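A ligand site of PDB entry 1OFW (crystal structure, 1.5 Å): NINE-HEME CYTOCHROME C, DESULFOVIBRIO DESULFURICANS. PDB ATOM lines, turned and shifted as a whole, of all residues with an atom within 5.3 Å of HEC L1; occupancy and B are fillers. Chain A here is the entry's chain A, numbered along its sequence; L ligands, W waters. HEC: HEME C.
NE2 of His 40 is bound to FE of HEC L2, at 2.0 Å.
SG of Cys 59 is covalently linked to CAB of HEC L3 (1.8 Å).
O2A of HEC L1 sits at hydrogen-bond distance from N of Ser 58 (3.2 Å).
NE2 of His 37 is bound to FE of HEC L1 (2.0 Å).
SG of Cys 50 is bonded to CAC of HEC L1.
A ring nitrogen (NE2) of His 51 is bound to an iron atom (FE) of HEC L1, at 2.0 Å.
A carbon (CAB) of HEC L1 is bonded to the side-chain sulfur of Cys 47 (1.8 Å).
Water W7 bridges an oxygen (O1D) of HEC L1 (2.5 Å) and the side-chain hydroxyl (OG) of Ser 60 (2.6 Å).
Water W1 lies within hydrogen-bond range of an oxygen (O2D) of HEC L1 and the backbone carbonyl oxygen (O) of Val 15.
Ser 8 touches HEC L1.
Ala 10 touches HEC L1 (CB to C4A, 3.6 Å).
Ile 14 touches HEC L1.
CE of Met 16 touches O1D of HEC L1, 3.7 Å away.
CE2 of Phe 35 touches C2D of HEC L1, 3.6 Å away.
His 40 touches HEC L1.
Ile 44 touches HEC L1 (CG2 to CMC, 3.6 Å).
Asn 46 touches HEC L1 (O to CMC, 3.97 Å).
O of Pro 56 touches CBA of HEC L1 (3.6 Å).
Val 57 touches HEC L1.
Cys 59 touches HEC L1 (N to CBD, 3.96 Å).
The side-chain carboxylate of Glu 41 sits at hydrogen-bond distance from a ring nitrogen (ND1) of His 37 (2.8 Å).
The side-chain carboxylate of Glu 41 sits at hydrogen-bond distance from the side-chain hydroxyl of Ser 8.
The backbone carbonyl oxygen (O) of Ile 14 is in hydrogen-bond range of the backbone NH (N) of Phe 35, 2.9 Å away.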
ATOM      1  N   SER A   8       0.052 -20.900  -4.483  1.00  0.00           N
ATOM      2  CA  SER A   8      -1.163 -20.560  -3.758  1.00  0.00           C
ATOM      3  C   SER A   8      -1.904 -19.356  -4.331  1.00  0.00           C
ATOM      4  O   SER A   8      -3.111 -19.253  -4.084  1.00  0.00           O
ATOM      5  CB  SER A   8      -0.838 -20.243  -2.302  1.00  0.00           C
ATOM      6  OG  SER A   8       0.220 -19.331  -2.163  1.00  0.00           O
ATOM      7  N   GLY A   9      -1.222 -18.450  -5.014  1.00  0.00           N
ATOM      8  CA  GLY A   9      -1.775 -17.191  -5.469  1.00  0.00           C
ATOM      9  C   GLY A   9      -1.658 -16.050  -4.503  1.00  0.00           C
ATOM     10  O   GLY A   9      -2.095 -14.929  -4.669  1.00  0.00           O
ATOM     11  N   ALA A  10      -1.086 -16.211  -3.325  1.00  0.00           N
ATOM     12  CA  ALA A  10      -0.537 -15.258  -2.404  1.00  0.00           C
ATOM     13  C   ALA A  10       0.628 -14.551  -3.058  1.00  0.00           C
ATOM     14  O   ALA A  10       1.291 -15.105  -3.935  1.00  0.00           O
ATOM     15  CB  ALA A  10      -0.031 -15.871  -1.092  1.00  0.00           C
ATOM     16  N   PRO A  11       0.911 -13.317  -2.662  1.00  0.00           N
ATOM     17  CA  PRO A  11       2.090 -12.666  -3.198  1.00  0.00           C
ATOM     18  C   PRO A  11       3.327 -13.429  -2.723  1.00  0.00           C
ATOM     19  O   PRO A  11       3.307 -14.063  -1.673  1.00  0.00           O
ATOM     20  CB  PRO A  11       2.018 -11.268  -2.631  1.00  0.00           C
ATOM     21  CG  PRO A  11       0.593 -11.089  -2.219  1.00  0.00           C
ATOM     22  CD  PRO A  11       0.162 -12.466  -1.741  1.00  0.00           C
ATOM     23  N   ILE A  14       5.551 -10.159   0.810  1.00  0.00           N
ATOM     24  CA  ILE A  14       4.492  -9.310   1.296  1.00  0.00           C
ATOM     25  C   ILE A  14       5.037  -8.335   2.327  1.00  0.00           C
ATOM     26  O   ILE A  14       5.573  -8.830   3.314  1.00  0.00           O
ATOM     27  CB  ILE A  14       3.369 -10.166   1.985  1.00  0.00           C
ATOM     28  CG1 ILE A  14       2.741 -11.209   1.061  1.00  0.00           C
ATOM     29  CG2 ILE A  14       2.319  -9.273   2.642  1.00  0.00           C
ATOM     30  CD1 ILE A  14       1.948 -12.323   1.723  1.00  0.00           C
ATOM     31  N   VAL A  15       4.870  -7.038   2.161  1.00  0.00           N
ATOM     32  CA  VAL A  15       5.133  -6.112   3.260  1.00  0.00           C
ATOM     33  C   VAL A  15       3.913  -6.087   4.203  1.00  0.00           C
ATOM     34  O   VAL A  15       2.783  -5.831   3.765  1.00  0.00           O
ATOM     35  CB  VAL A  15       5.410  -4.681   2.811  1.00  0.00           C
ATOM     36  CG1 VAL A  15       5.919  -3.871   3.986  1.00  0.00           C
ATOM     37  CG2 VAL A  15       6.436  -4.640   1.666  1.00  0.00           C
ATOM     38  N   MET A  16       4.138  -6.336   5.483  1.00  0.00           N
ATOM     39  CA  MET A  16       3.176  -6.311   6.547  1.00  0.00           C
ATOM     40  C   MET A  16       3.364  -5.076   7.400  1.00  0.00           C
ATOM     41  O   MET A  16       4.426  -4.790   7.969  1.00  0.00           O
ATOM     42  CB  MET A  16       3.297  -7.568   7.423  1.00  0.00           C
ATOM     43  CG  MET A  16       3.143  -8.861   6.620  1.00  0.00           C
ATOM     44  SD  MET A  16       3.438 -10.345   7.595  1.00  0.00           S
ATOM     45  CE  MET A  16       2.027 -10.318   8.681  1.00  0.00           C
ATOM     46  N   PHE A  35       7.508 -10.522   4.659  1.00  0.00           N
ATOM     47  CA  PHE A  35       7.245 -11.917   4.867  1.00  0.00           C
ATOM     48  C   PHE A  35       7.371 -12.634   3.530  1.00  0.00           C
ATOM     49  O   PHE A  35       6.705 -12.263   2.566  1.00  0.00           O
ATOM     50  CB  PHE A  35       5.838 -12.097   5.448  1.00  0.00           C
ATOM     51  CG  PHE A  35       5.433 -13.545   5.601  1.00  0.00           C
ATOM     52  CD1 PHE A  35       6.008 -14.350   6.577  1.00  0.00           C
ATOM     53  CD2 PHE A  35       4.499 -14.141   4.781  1.00  0.00           C
ATOM     54  CE1 PHE A  35       5.662 -15.657   6.751  1.00  0.00           C
ATOM     55  CE2 PHE A  35       4.157 -15.458   4.968  1.00  0.00           C
ATOM     56  CZ  PHE A  35       4.728 -16.264   5.922  1.00  0.00           C
ATOM     57  N   HIS A  37       6.334 -15.373   1.584  1.00  0.00           N
ATOM     58  CA  HIS A  37       5.271 -16.348   1.547  1.00  0.00           C
ATOM     59  C   HIS A  37       5.687 -17.575   0.749  1.00  0.00           C
ATOM     60  O   HIS A  37       5.333 -18.696   1.076  1.00  0.00           O
ATOM     61  CB  HIS A  37       3.988 -15.716   0.979  1.00  0.00           C
ATOM     62  CG  HIS A  37       2.746 -16.459   1.330  1.00  0.00           C
ATOM     63  ND1 HIS A  37       2.348 -17.649   0.775  1.00  0.00           N
ATOM     64  CD2 HIS A  37       1.777 -16.190   2.258  1.00  0.00           C
ATOM     65  CE1 HIS A  37       1.209 -18.048   1.320  1.00  0.00           C
ATOM     66  NE2 HIS A  37       0.836 -17.172   2.240  1.00  0.00           N
ATOM     67  N   HIS A  40       7.703 -19.910   2.846  1.00  0.00           N
ATOM     68  CA  HIS A  40       6.906 -20.554   3.875  1.00  0.00           C
ATOM     69  C   HIS A  40       5.905 -21.568   3.308  1.00  0.00           C
ATOM     70  O   HIS A  40       5.772 -22.670   3.828  1.00  0.00           O
ATOM     71  CB  HIS A  40       6.179 -19.496   4.714  1.00  0.00           C
ATOM     72  CG  HIS A  40       7.087 -18.843   5.726  1.00  0.00           C
ATOM     73  ND1 HIS A  40       7.937 -17.796   5.442  1.00  0.00           N
ATOM     74  CD2 HIS A  40       7.234 -19.094   7.051  1.00  0.00           C
ATOM     75  CE1 HIS A  40       8.587 -17.451   6.541  1.00  0.00           C
ATOM     76  NE2 HIS A  40       8.175 -18.216   7.533  1.00  0.00           N
ATOM     77  N   GLU A  41       5.204 -21.294   2.206  1.00  0.00           N
ATOM     78  CA  GLU A  41       4.219 -22.254   1.717  1.00  0.00           C
ATOM     79  C   GLU A  41       4.933 -23.472   1.141  1.00  0.00           C
ATOM     80  O   GLU A  41       4.300 -24.533   1.135  1.00  0.00           O
ATOM     81  CB  GLU A  41       3.271 -21.592   0.721  1.00  0.00           C
ATOM     82  CG  GLU A  41       3.848 -21.332  -0.668  1.00  0.00           C
ATOM     83  CD  GLU A  41       2.791 -20.690  -1.570  1.00  0.00           C
ATOM     84  OE1 GLU A  41       2.416 -19.526  -1.293  1.00  0.00           O
ATOM     85  OE2 GLU A  41       2.302 -21.338  -2.529  1.00  0.00           O
ATOM     86  N   ILE A  44       5.711 -25.459   4.746  1.00  0.00           N
ATOM     87  CA  ILE A  44       4.619 -25.702   5.639  1.00  0.00           C
ATOM     88  C   ILE A  44       3.399 -26.145   4.769  1.00  0.00           C
ATOM     89  O   ILE A  44       2.891 -25.310   4.011  1.00  0.00           O
ATOM     90  CB  ILE A  44       4.304 -24.482   6.493  1.00  0.00           C
ATOM     91  CG1 ILE A  44       5.473 -23.922   7.321  1.00  0.00           C
ATOM     92  CG2 ILE A  44       3.112 -24.756   7.399  1.00  0.00           C
ATOM     93  CD1 ILE A  44       6.126 -24.939   8.216  1.00  0.00           C
ATOM     94  N   ASP A  45       2.973 -27.390   4.872  1.00  0.00           N
ATOM     95  CA  ASP A  45       2.041 -27.987   3.927  1.00  0.00           C
ATOM     96  C   ASP A  45       0.623 -27.443   3.977  1.00  0.00           C
ATOM     97  O   ASP A  45      -0.052 -27.210   2.972  1.00  0.00           O
ATOM     98  CB  ASP A  45       1.962 -29.504   4.157  1.00  0.00           C
ATOM     99  CG  ASP A  45       3.303 -30.194   4.301  1.00  0.00           C
ATOM    100  OD1 ASP A  45       3.688 -30.938   3.361  1.00  0.00           O
ATOM    101  OD2 ASP A  45       3.970 -30.019   5.350  1.00  0.00           O
ATOM    102  N   ASN A  46       0.130 -27.261   5.196  1.00  0.00           N
ATOM    103  CA  ASN A  46      -1.261 -26.912   5.400  1.00  0.00           C
ATOM    104  C   ASN A  46      -1.449 -25.411   5.528  1.00  0.00           C
ATOM    105  O   ASN A  46      -0.929 -24.816   6.472  1.00  0.00           O
ATOM    106  CB  ASN A  46      -1.754 -27.588   6.701  1.00  0.00           C
ATOM    107  CG  ASN A  46      -3.240 -27.514   6.909  1.00  0.00           C
ATOM    108  OD1 ASN A  46      -3.935 -26.569   6.548  1.00  0.00           O
ATOM    109  ND2 ASN A  46      -3.814 -28.545   7.535  1.00  0.00           N
ATOM    110  N   CYS A  47      -2.173 -24.807   4.594  1.00  0.00           N
ATOM    111  CA  CYS A  47      -2.475 -23.392   4.648  1.00  0.00           C
ATOM    112  C   CYS A  47      -3.072 -22.985   5.981  1.00  0.00           C
ATOM    113  O   CYS A  47      -2.767 -21.885   6.498  1.00  0.00           O
ATOM    114  CB  CYS A  47      -3.469 -23.010   3.554  1.00  0.00           C
ATOM    115  SG  CYS A  47      -3.048 -23.506   1.905  1.00  0.00           S
ATOM    116  N   CYS A  50      -1.370 -21.704   9.461  1.00  0.00           N
ATOM    117  CA  CYS A  50      -1.259 -20.273   9.680  1.00  0.00           C
ATOM    118  C   CYS A  50      -2.595 -19.557   9.585  1.00  0.00           C
ATOM    119  O   CYS A  50      -2.932 -18.791  10.490  1.00  0.00           O
ATOM    120  CB  CYS A  50      -0.269 -19.712   8.647  1.00  0.00           C
ATOM    121  SG  CYS A  50       1.365 -20.463   8.838  1.00  0.00           S
ATOM    122  N   HIS A  51      -3.304 -19.809   8.487  1.00  0.00           N
ATOM    123  CA  HIS A  51      -4.588 -19.151   8.299  1.00  0.00           C
ATOM    124  C   HIS A  51      -5.648 -19.934   9.073  1.00  0.00           C
ATOM    125  O   HIS A  51      -6.470 -20.649   8.496  1.00  0.00           O
ATOM    126  CB  HIS A  51      -4.936 -19.040   6.807  1.00  0.00           C
ATOM    127  CG  HIS A  51      -3.926 -18.252   6.021  1.00  0.00           C
ATOM    128  ND1 HIS A  51      -3.902 -16.895   6.045  1.00  0.00           N
ATOM    129  CD2 HIS A  51      -2.937 -18.656   5.183  1.00  0.00           C
ATOM    130  CE1 HIS A  51      -2.925 -16.477   5.252  1.00  0.00           C
ATOM    131  NE2 HIS A  51      -2.320 -17.507   4.723  1.00  0.00           N
ATOM    132  N   PRO A  56      -8.260 -17.237   3.710  1.00  0.00           N
ATOM    133  CA  PRO A  56      -6.913 -16.868   3.238  1.00  0.00           C
ATOM    134  C   PRO A  56      -6.843 -15.373   3.094  1.00  0.00           C
ATOM    135  O   PRO A  56      -6.771 -14.811   2.017  1.00  0.00           O
ATOM    136  CB  PRO A  56      -6.833 -17.572   1.889  1.00  0.00           C
ATOM    137  CG  PRO A  56      -8.253 -17.481   1.381  1.00  0.00           C
ATOM    138  CD  PRO A  56      -9.165 -17.522   2.583  1.00  0.00           C
ATOM    139  N   VAL A  57      -6.830 -14.718   4.254  1.00  0.00           N
ATOM    140  CA  VAL A  57      -6.899 -13.288   4.380  1.00  0.00           C
ATOM    141  C   VAL A  57      -5.813 -12.744   5.297  1.00  0.00           C
ATOM    142  O   VAL A  57      -5.344 -13.504   6.157  1.00  0.00           O
ATOM    143  CB  VAL A  57      -8.294 -12.798   4.830  1.00  0.00           C
ATOM    144  CG1 VAL A  57      -8.496 -12.896   6.329  1.00  0.00           C
ATOM    145  CG2 VAL A  57      -8.516 -11.361   4.389  1.00  0.00           C
ATOM    146  N   SER A  58      -5.452 -11.507   5.107  1.00  0.00           N
ATOM    147  CA  SER A  58      -4.382 -10.956   5.935  1.00  0.00           C
ATOM    148  C   SER A  58      -4.766 -10.997   7.413  1.00  0.00           C
ATOM    149  O   SER A  58      -5.902 -10.757   7.788  1.00  0.00           O
ATOM    150  CB  SER A  58      -4.048  -9.583   5.414  1.00  0.00           C
ATOM    151  OG  SER A  58      -4.953  -8.601   5.840  1.00  0.00           O
ATOM    152  N   CYS A  59      -3.775 -11.350   8.242  1.00  0.00           N
ATOM    153  CA  CYS A  59      -4.018 -11.430   9.676  1.00  0.00           C
ATOM    154  C   CYS A  59      -4.556 -10.123  10.225  1.00  0.00           C
ATOM    155  O   CYS A  59      -5.402 -10.140  11.136  1.00  0.00           O
ATOM    156  CB  CYS A  59      -2.732 -11.790  10.449  1.00  0.00           C
ATOM    157  SG  CYS A  59      -1.724 -13.078   9.713  1.00  0.00           S
ATOM    158  N   SER A  60      -4.093  -9.000   9.745  1.00  0.00           N
ATOM    159  CA  SER A  60      -4.470  -7.705  10.281  1.00  0.00           C
ATOM    160  C   SER A  60      -5.935  -7.390   9.985  1.00  0.00           C
ATOM    161  O   SER A  60      -6.440  -6.401  10.533  1.00  0.00           O
ATOM    162  CB  SER A  60      -3.613  -6.536   9.759  1.00  0.00           C
ATOM    163  OG  SER A  60      -3.462  -6.603   8.339  1.00  0.00           O
HETATM  164 FE   HEC L   1      -0.751 -17.318   3.460  1.00  0.00          FE
HETATM  165  CHA HEC L   1      -1.011 -13.943   3.160  1.00  0.00           C
HETATM  166  CHB HEC L   1      -3.023 -17.760   0.945  1.00  0.00           C
HETATM  167  CHC HEC L   1      -0.073 -20.650   3.433  1.00  0.00           C
HETATM  168  CHD HEC L   1       1.100 -16.948   6.318  1.00  0.00           C
HETATM  169  NA  HEC L   1      -1.803 -16.109   2.306  1.00  0.00           N
HETATM  170  C1A HEC L   1      -1.754 -14.731   2.302  1.00  0.00           C
HETATM  171  C2A HEC L   1      -2.650 -14.217   1.270  1.00  0.00           C
HETATM  172  C3A HEC L   1      -3.216 -15.281   0.677  1.00  0.00           C
HETATM  173  C4A HEC L   1      -2.693 -16.471   1.311  1.00  0.00           C
HETATM  174  CMA HEC L   1      -4.229 -15.343  -0.481  1.00  0.00           C
HETATM  175  CAA HEC L   1      -2.919 -12.729   0.977  1.00  0.00           C
HETATM  176  CBA HEC L   1      -4.163 -12.348   1.812  1.00  0.00           C
HETATM  177  CGA HEC L   1      -4.516 -10.892   1.899  1.00  0.00           C
HETATM  178  O1A HEC L   1      -3.657 -10.000   1.800  1.00  0.00           O
HETATM  179  O2A HEC L   1      -5.747 -10.639   2.084  1.00  0.00           O
HETATM  180  NB  HEC L   1      -1.457 -18.884   2.441  1.00  0.00           N
HETATM  181  C1B HEC L   1      -2.417 -18.886   1.431  1.00  0.00           C
HETATM  182  C2B HEC L   1      -2.657 -20.253   1.005  1.00  0.00           C
HETATM  183  C3B HEC L   1      -1.794 -21.056   1.651  1.00  0.00           C
HETATM  184  C4B HEC L   1      -1.039 -20.183   2.560  1.00  0.00           C
HETATM  185  CMB HEC L   1      -3.730 -20.634  -0.050  1.00  0.00           C
HETATM  186  CAB HEC L   1      -1.543 -22.555   1.537  1.00  0.00           C
HETATM  187  CBB HEC L   1      -1.094 -22.983   0.132  1.00  0.00           C
HETATM  188  NC  HEC L   1       0.289 -18.541   4.645  1.00  0.00           N
HETATM  189  C1C HEC L   1       0.454 -19.880   4.464  1.00  0.00           C
HETATM  190  C2C HEC L   1       1.273 -20.420   5.513  1.00  0.00           C
HETATM  191  C3C HEC L   1       1.570 -19.414   6.346  1.00  0.00           C
HETATM  192  C4C HEC L   1       0.980 -18.214   5.809  1.00  0.00           C
HETATM  193  CMC HEC L   1       1.650 -21.916   5.645  1.00  0.00           C
HETATM  194  CAC HEC L   1       2.316 -19.426   7.684  1.00  0.00           C
HETATM  195  CBC HEC L   1       3.730 -20.023   7.631  1.00  0.00           C
HETATM  196  ND  HEC L   1      -0.136 -15.768   4.555  1.00  0.00           N
HETATM  197  C1D HEC L   1       0.633 -15.806   5.705  1.00  0.00           C
HETATM  198  C2D HEC L   1       0.917 -14.464   6.135  1.00  0.00           C
HETATM  199  C3D HEC L   1       0.402 -13.620   5.218  1.00  0.00           C
HETATM  200  C4D HEC L   1      -0.288 -14.447   4.244  1.00  0.00           C
HETATM  201  CMD HEC L   1       1.704 -14.155   7.438  1.00  0.00           C
HETATM  202  CAD HEC L   1       0.510 -12.097   5.161  1.00  0.00           C
HETATM  203  CBD HEC L   1      -0.755 -11.369   5.673  1.00  0.00           C
HETATM  204  CGD HEC L   1      -0.550  -9.835   5.511  1.00  0.00           C
HETATM  205  O1D HEC L   1      -0.774  -9.177   6.554  1.00  0.00           O
HETATM  206  O2D HEC L   1      -0.225  -9.336   4.430  1.00  0.00           O
HETATM  207 FE   HEC L   2       8.916 -18.239   9.413  1.00  0.00          FE
HETATM  208  CHA HEC L   2      11.763 -19.083   7.807  1.00  0.00           C
HETATM  209  CHB HEC L   2       9.792 -14.898   9.234  1.00  0.00           C
HETATM  210  CHC HEC L   2       5.799 -17.365  10.400  1.00  0.00           C
HETATM  211  CHD HEC L   2       8.132 -21.548   9.806  1.00  0.00           C
HETATM  212  NA  HEC L   2      10.510 -17.218   8.763  1.00  0.00           N
HETATM  213  C1A HEC L   2      11.617 -17.738   8.117  1.00  0.00           C
HETATM  214  C2A HEC L   2      12.532 -16.668   7.855  1.00  0.00           C
HETATM  215  C3A HEC L   2      12.039 -15.539   8.361  1.00  0.00           C
HETATM  216  C4A HEC L   2      10.689 -15.855   8.822  1.00  0.00           C
HETATM  217  CMA HEC L   2      12.676 -14.176   8.442  1.00  0.00           C
HETATM  218  CAA HEC L   2      13.866 -16.853   7.069  1.00  0.00           C
HETATM  219  CBA HEC L   2      13.607 -17.080   5.551  1.00  0.00           C
HETATM  220  CGA HEC L   2      12.892 -15.841   4.999  1.00  0.00           C
HETATM  221  O1A HEC L   2      13.579 -14.831   4.871  1.00  0.00           O
HETATM  222  O2A HEC L   2      11.657 -15.954   4.766  1.00  0.00           O
HETATM  223  NB  HEC L   2       7.998 -16.490   9.748  1.00  0.00           N
HETATM  224  C1B HEC L   2       8.483 -15.194   9.608  1.00  0.00           C
HETATM  225  C2B HEC L   2       7.451 -14.233   9.925  1.00  0.00           C
HETATM  226  C3B HEC L   2       6.342 -14.935  10.268  1.00  0.00           C
HETATM  227  C4B HEC L   2       6.674 -16.325  10.133  1.00  0.00           C
HETATM  228  CMB HEC L   2       7.662 -12.722   9.873  1.00  0.00           C
HETATM  229  CAB HEC L   2       4.962 -14.468  10.756  1.00  0.00           C
HETATM  230  CBB HEC L   2       4.303 -13.375   9.847  1.00  0.00           C
HETATM  231  NC  HEC L   2       7.305 -19.260  10.007  1.00  0.00           N
HETATM  232  C1C HEC L   2       6.085 -18.713  10.435  1.00  0.00           C
HETATM  233  C2C HEC L   2       5.227 -19.781  10.919  1.00  0.00           C
HETATM  234  C3C HEC L   2       5.873 -20.930  10.732  1.00  0.00           C
HETATM  235  C4C HEC L   2       7.166 -20.616  10.164  1.00  0.00           C
HETATM  236  CMC HEC L   2       3.860 -19.471  11.572  1.00  0.00           C
HETATM  237  CAC HEC L   2       5.497 -22.359  11.075  1.00  0.00           C
HETATM  238  CBC HEC L   2       3.986 -22.713  11.028  1.00  0.00           C
HETATM  239  ND  HEC L   2       9.772 -19.963   8.904  1.00  0.00           N
HETATM  240  C1D HEC L   2       9.297 -21.231   9.156  1.00  0.00           C
HETATM  241  C2D HEC L   2      10.214 -22.207   8.617  1.00  0.00           C
HETATM  242  C3D HEC L   2      11.182 -21.529   7.975  1.00  0.00           C
HETATM  243  C4D HEC L   2      10.961 -20.114   8.204  1.00  0.00           C
HETATM  244  CMD HEC L   2      10.043 -23.712   8.761  1.00  0.00           C
HETATM  245  CAD HEC L   2      12.348 -22.065   7.138  1.00  0.00           C
HETATM  246  CBD HEC L   2      11.841 -22.444   5.724  1.00  0.00           C
HETATM  247  CGD HEC L   2      12.864 -23.236   4.928  1.00  0.00           C
HETATM  248  O1D HEC L   2      12.844 -23.178   3.676  1.00  0.00           O
HETATM  249  O2D HEC L   2      13.690 -23.935   5.549  1.00  0.00           O
HETATM  250 FE   HEC L   3      -5.920 -15.132  14.549  1.00  0.00          FE
HETATM  251  CHA HEC L   3      -6.387 -16.056  17.801  1.00  0.00           C
HETATM  252  CHB HEC L   3      -2.545 -15.489  14.895  1.00  0.00           C
HETATM  253  CHC HEC L   3      -5.527 -14.498  11.214  1.00  0.00           C
HETATM  254  CHD HEC L   3      -9.214 -14.325  14.321  1.00  0.00           C
HETATM  255  NA  HEC L   3      -4.722 -15.648  16.045  1.00  0.00           N
HETATM  256  C1A HEC L   3      -5.091 -16.029  17.335  1.00  0.00           C
HETATM  257  C2A HEC L   3      -3.912 -16.397  18.095  1.00  0.00           C
HETATM  258  C3A HEC L   3      -2.837 -16.171  17.284  1.00  0.00           C
HETATM  259  C4A HEC L   3      -3.335 -15.748  16.006  1.00  0.00           C
HETATM  260  CMA HEC L   3      -1.358 -16.403  17.621  1.00  0.00           C
HETATM  261  CAA HEC L   3      -3.869 -16.986  19.505  1.00  0.00           C
HETATM  262  CBA HEC L   3      -3.672 -15.883  20.569  1.00  0.00           C
HETATM  263  CGA HEC L   3      -3.675 -16.478  21.980  1.00  0.00           C
HETATM  264  O1A HEC L   3      -4.123 -17.644  22.168  1.00  0.00           O
HETATM  265  O2A HEC L   3      -3.196 -15.747  22.870  1.00  0.00           O
HETATM  266  NB  HEC L   3      -4.391 -15.066  13.297  1.00  0.00           N
HETATM  267  C1B HEC L   3      -3.060 -15.205  13.647  1.00  0.00           C
HETATM  268  C2B HEC L   3      -2.232 -15.084  12.444  1.00  0.00           C
HETATM  269  C3B HEC L   3      -3.037 -14.800  11.420  1.00  0.00           C
HETATM  270  C4B HEC L   3      -4.403 -14.776  11.956  1.00  0.00           C
HETATM  271  CMB HEC L   3      -0.705 -15.277  12.463  1.00  0.00           C
HETATM  272  CAB HEC L   3      -2.725 -14.566   9.944  1.00  0.00           C
HETATM  273  CBB HEC L   3      -1.883 -15.731   9.389  1.00  0.00           C
HETATM  274  NC  HEC L   3      -7.151 -14.615  13.055  1.00  0.00           N
HETATM  275  C1C HEC L   3      -6.796 -14.326  11.756  1.00  0.00           C
HETATM  276  C2C HEC L   3      -7.936 -13.822  11.003  1.00  0.00           C
HETATM  277  C3C HEC L   3      -8.961 -13.752  11.879  1.00  0.00           C
HETATM  278  C4C HEC L   3      -8.481 -14.244  13.144  1.00  0.00           C
HETATM  279  CMC HEC L   3      -7.850 -13.421   9.510  1.00  0.00           C
HETATM  280  CAC HEC L   3     -10.378 -13.158  11.672  1.00  0.00           C
HETATM  281  CBC HEC L   3     -11.150 -13.817  10.514  1.00  0.00           C
HETATM  282  ND  HEC L   3      -7.506 -15.321  15.756  1.00  0.00           N
HETATM  283  C1D HEC L   3      -8.797 -14.925  15.465  1.00  0.00           C
HETATM  284  C2D HEC L   3      -9.652 -15.289  16.579  1.00  0.00           C
HETATM  285  C3D HEC L   3      -8.885 -15.843  17.525  1.00  0.00           C
HETATM  286  C4D HEC L   3      -7.508 -15.757  17.067  1.00  0.00           C
HETATM  287  CMD HEC L   3     -11.180 -15.056  16.531  1.00  0.00           C
HETATM  288  CAD HEC L   3      -9.290 -16.513  18.866  1.00  0.00           C
HETATM  289  CBD HEC L   3      -9.509 -18.015  18.531  1.00  0.00           C
HETATM  290  CGD HEC L   3      -9.595 -18.941  19.729  1.00  0.00           C
HETATM  291  O1D HEC L   3      -9.669 -20.174  19.516  1.00  0.00           O
HETATM  292  O2D HEC L   3      -9.579 -18.387  20.845  1.00  0.00           O
HETATM  293  O   HOH W   1       0.139  -6.738   3.999  1.00  0.00           O
HETATM  294  O   HOH W   2      -1.026 -10.037   1.827  1.00  0.00           O
HETATM  295  O   HOH W   3       1.711 -25.017   0.321  1.00  0.00           O
HETATM  296  O   HOH W   4       1.035 -24.292   2.736  1.00  0.00           O
HETATM  297  O   HOH W   5      -7.928 -11.683   0.793  1.00  0.00           O
HETATM  298  O   HOH W   6      -3.879  -7.300   1.758  1.00  0.00           O
HETATM  299  O   HOH W   7      -1.152  -6.837   7.183  1.00  0.00           O
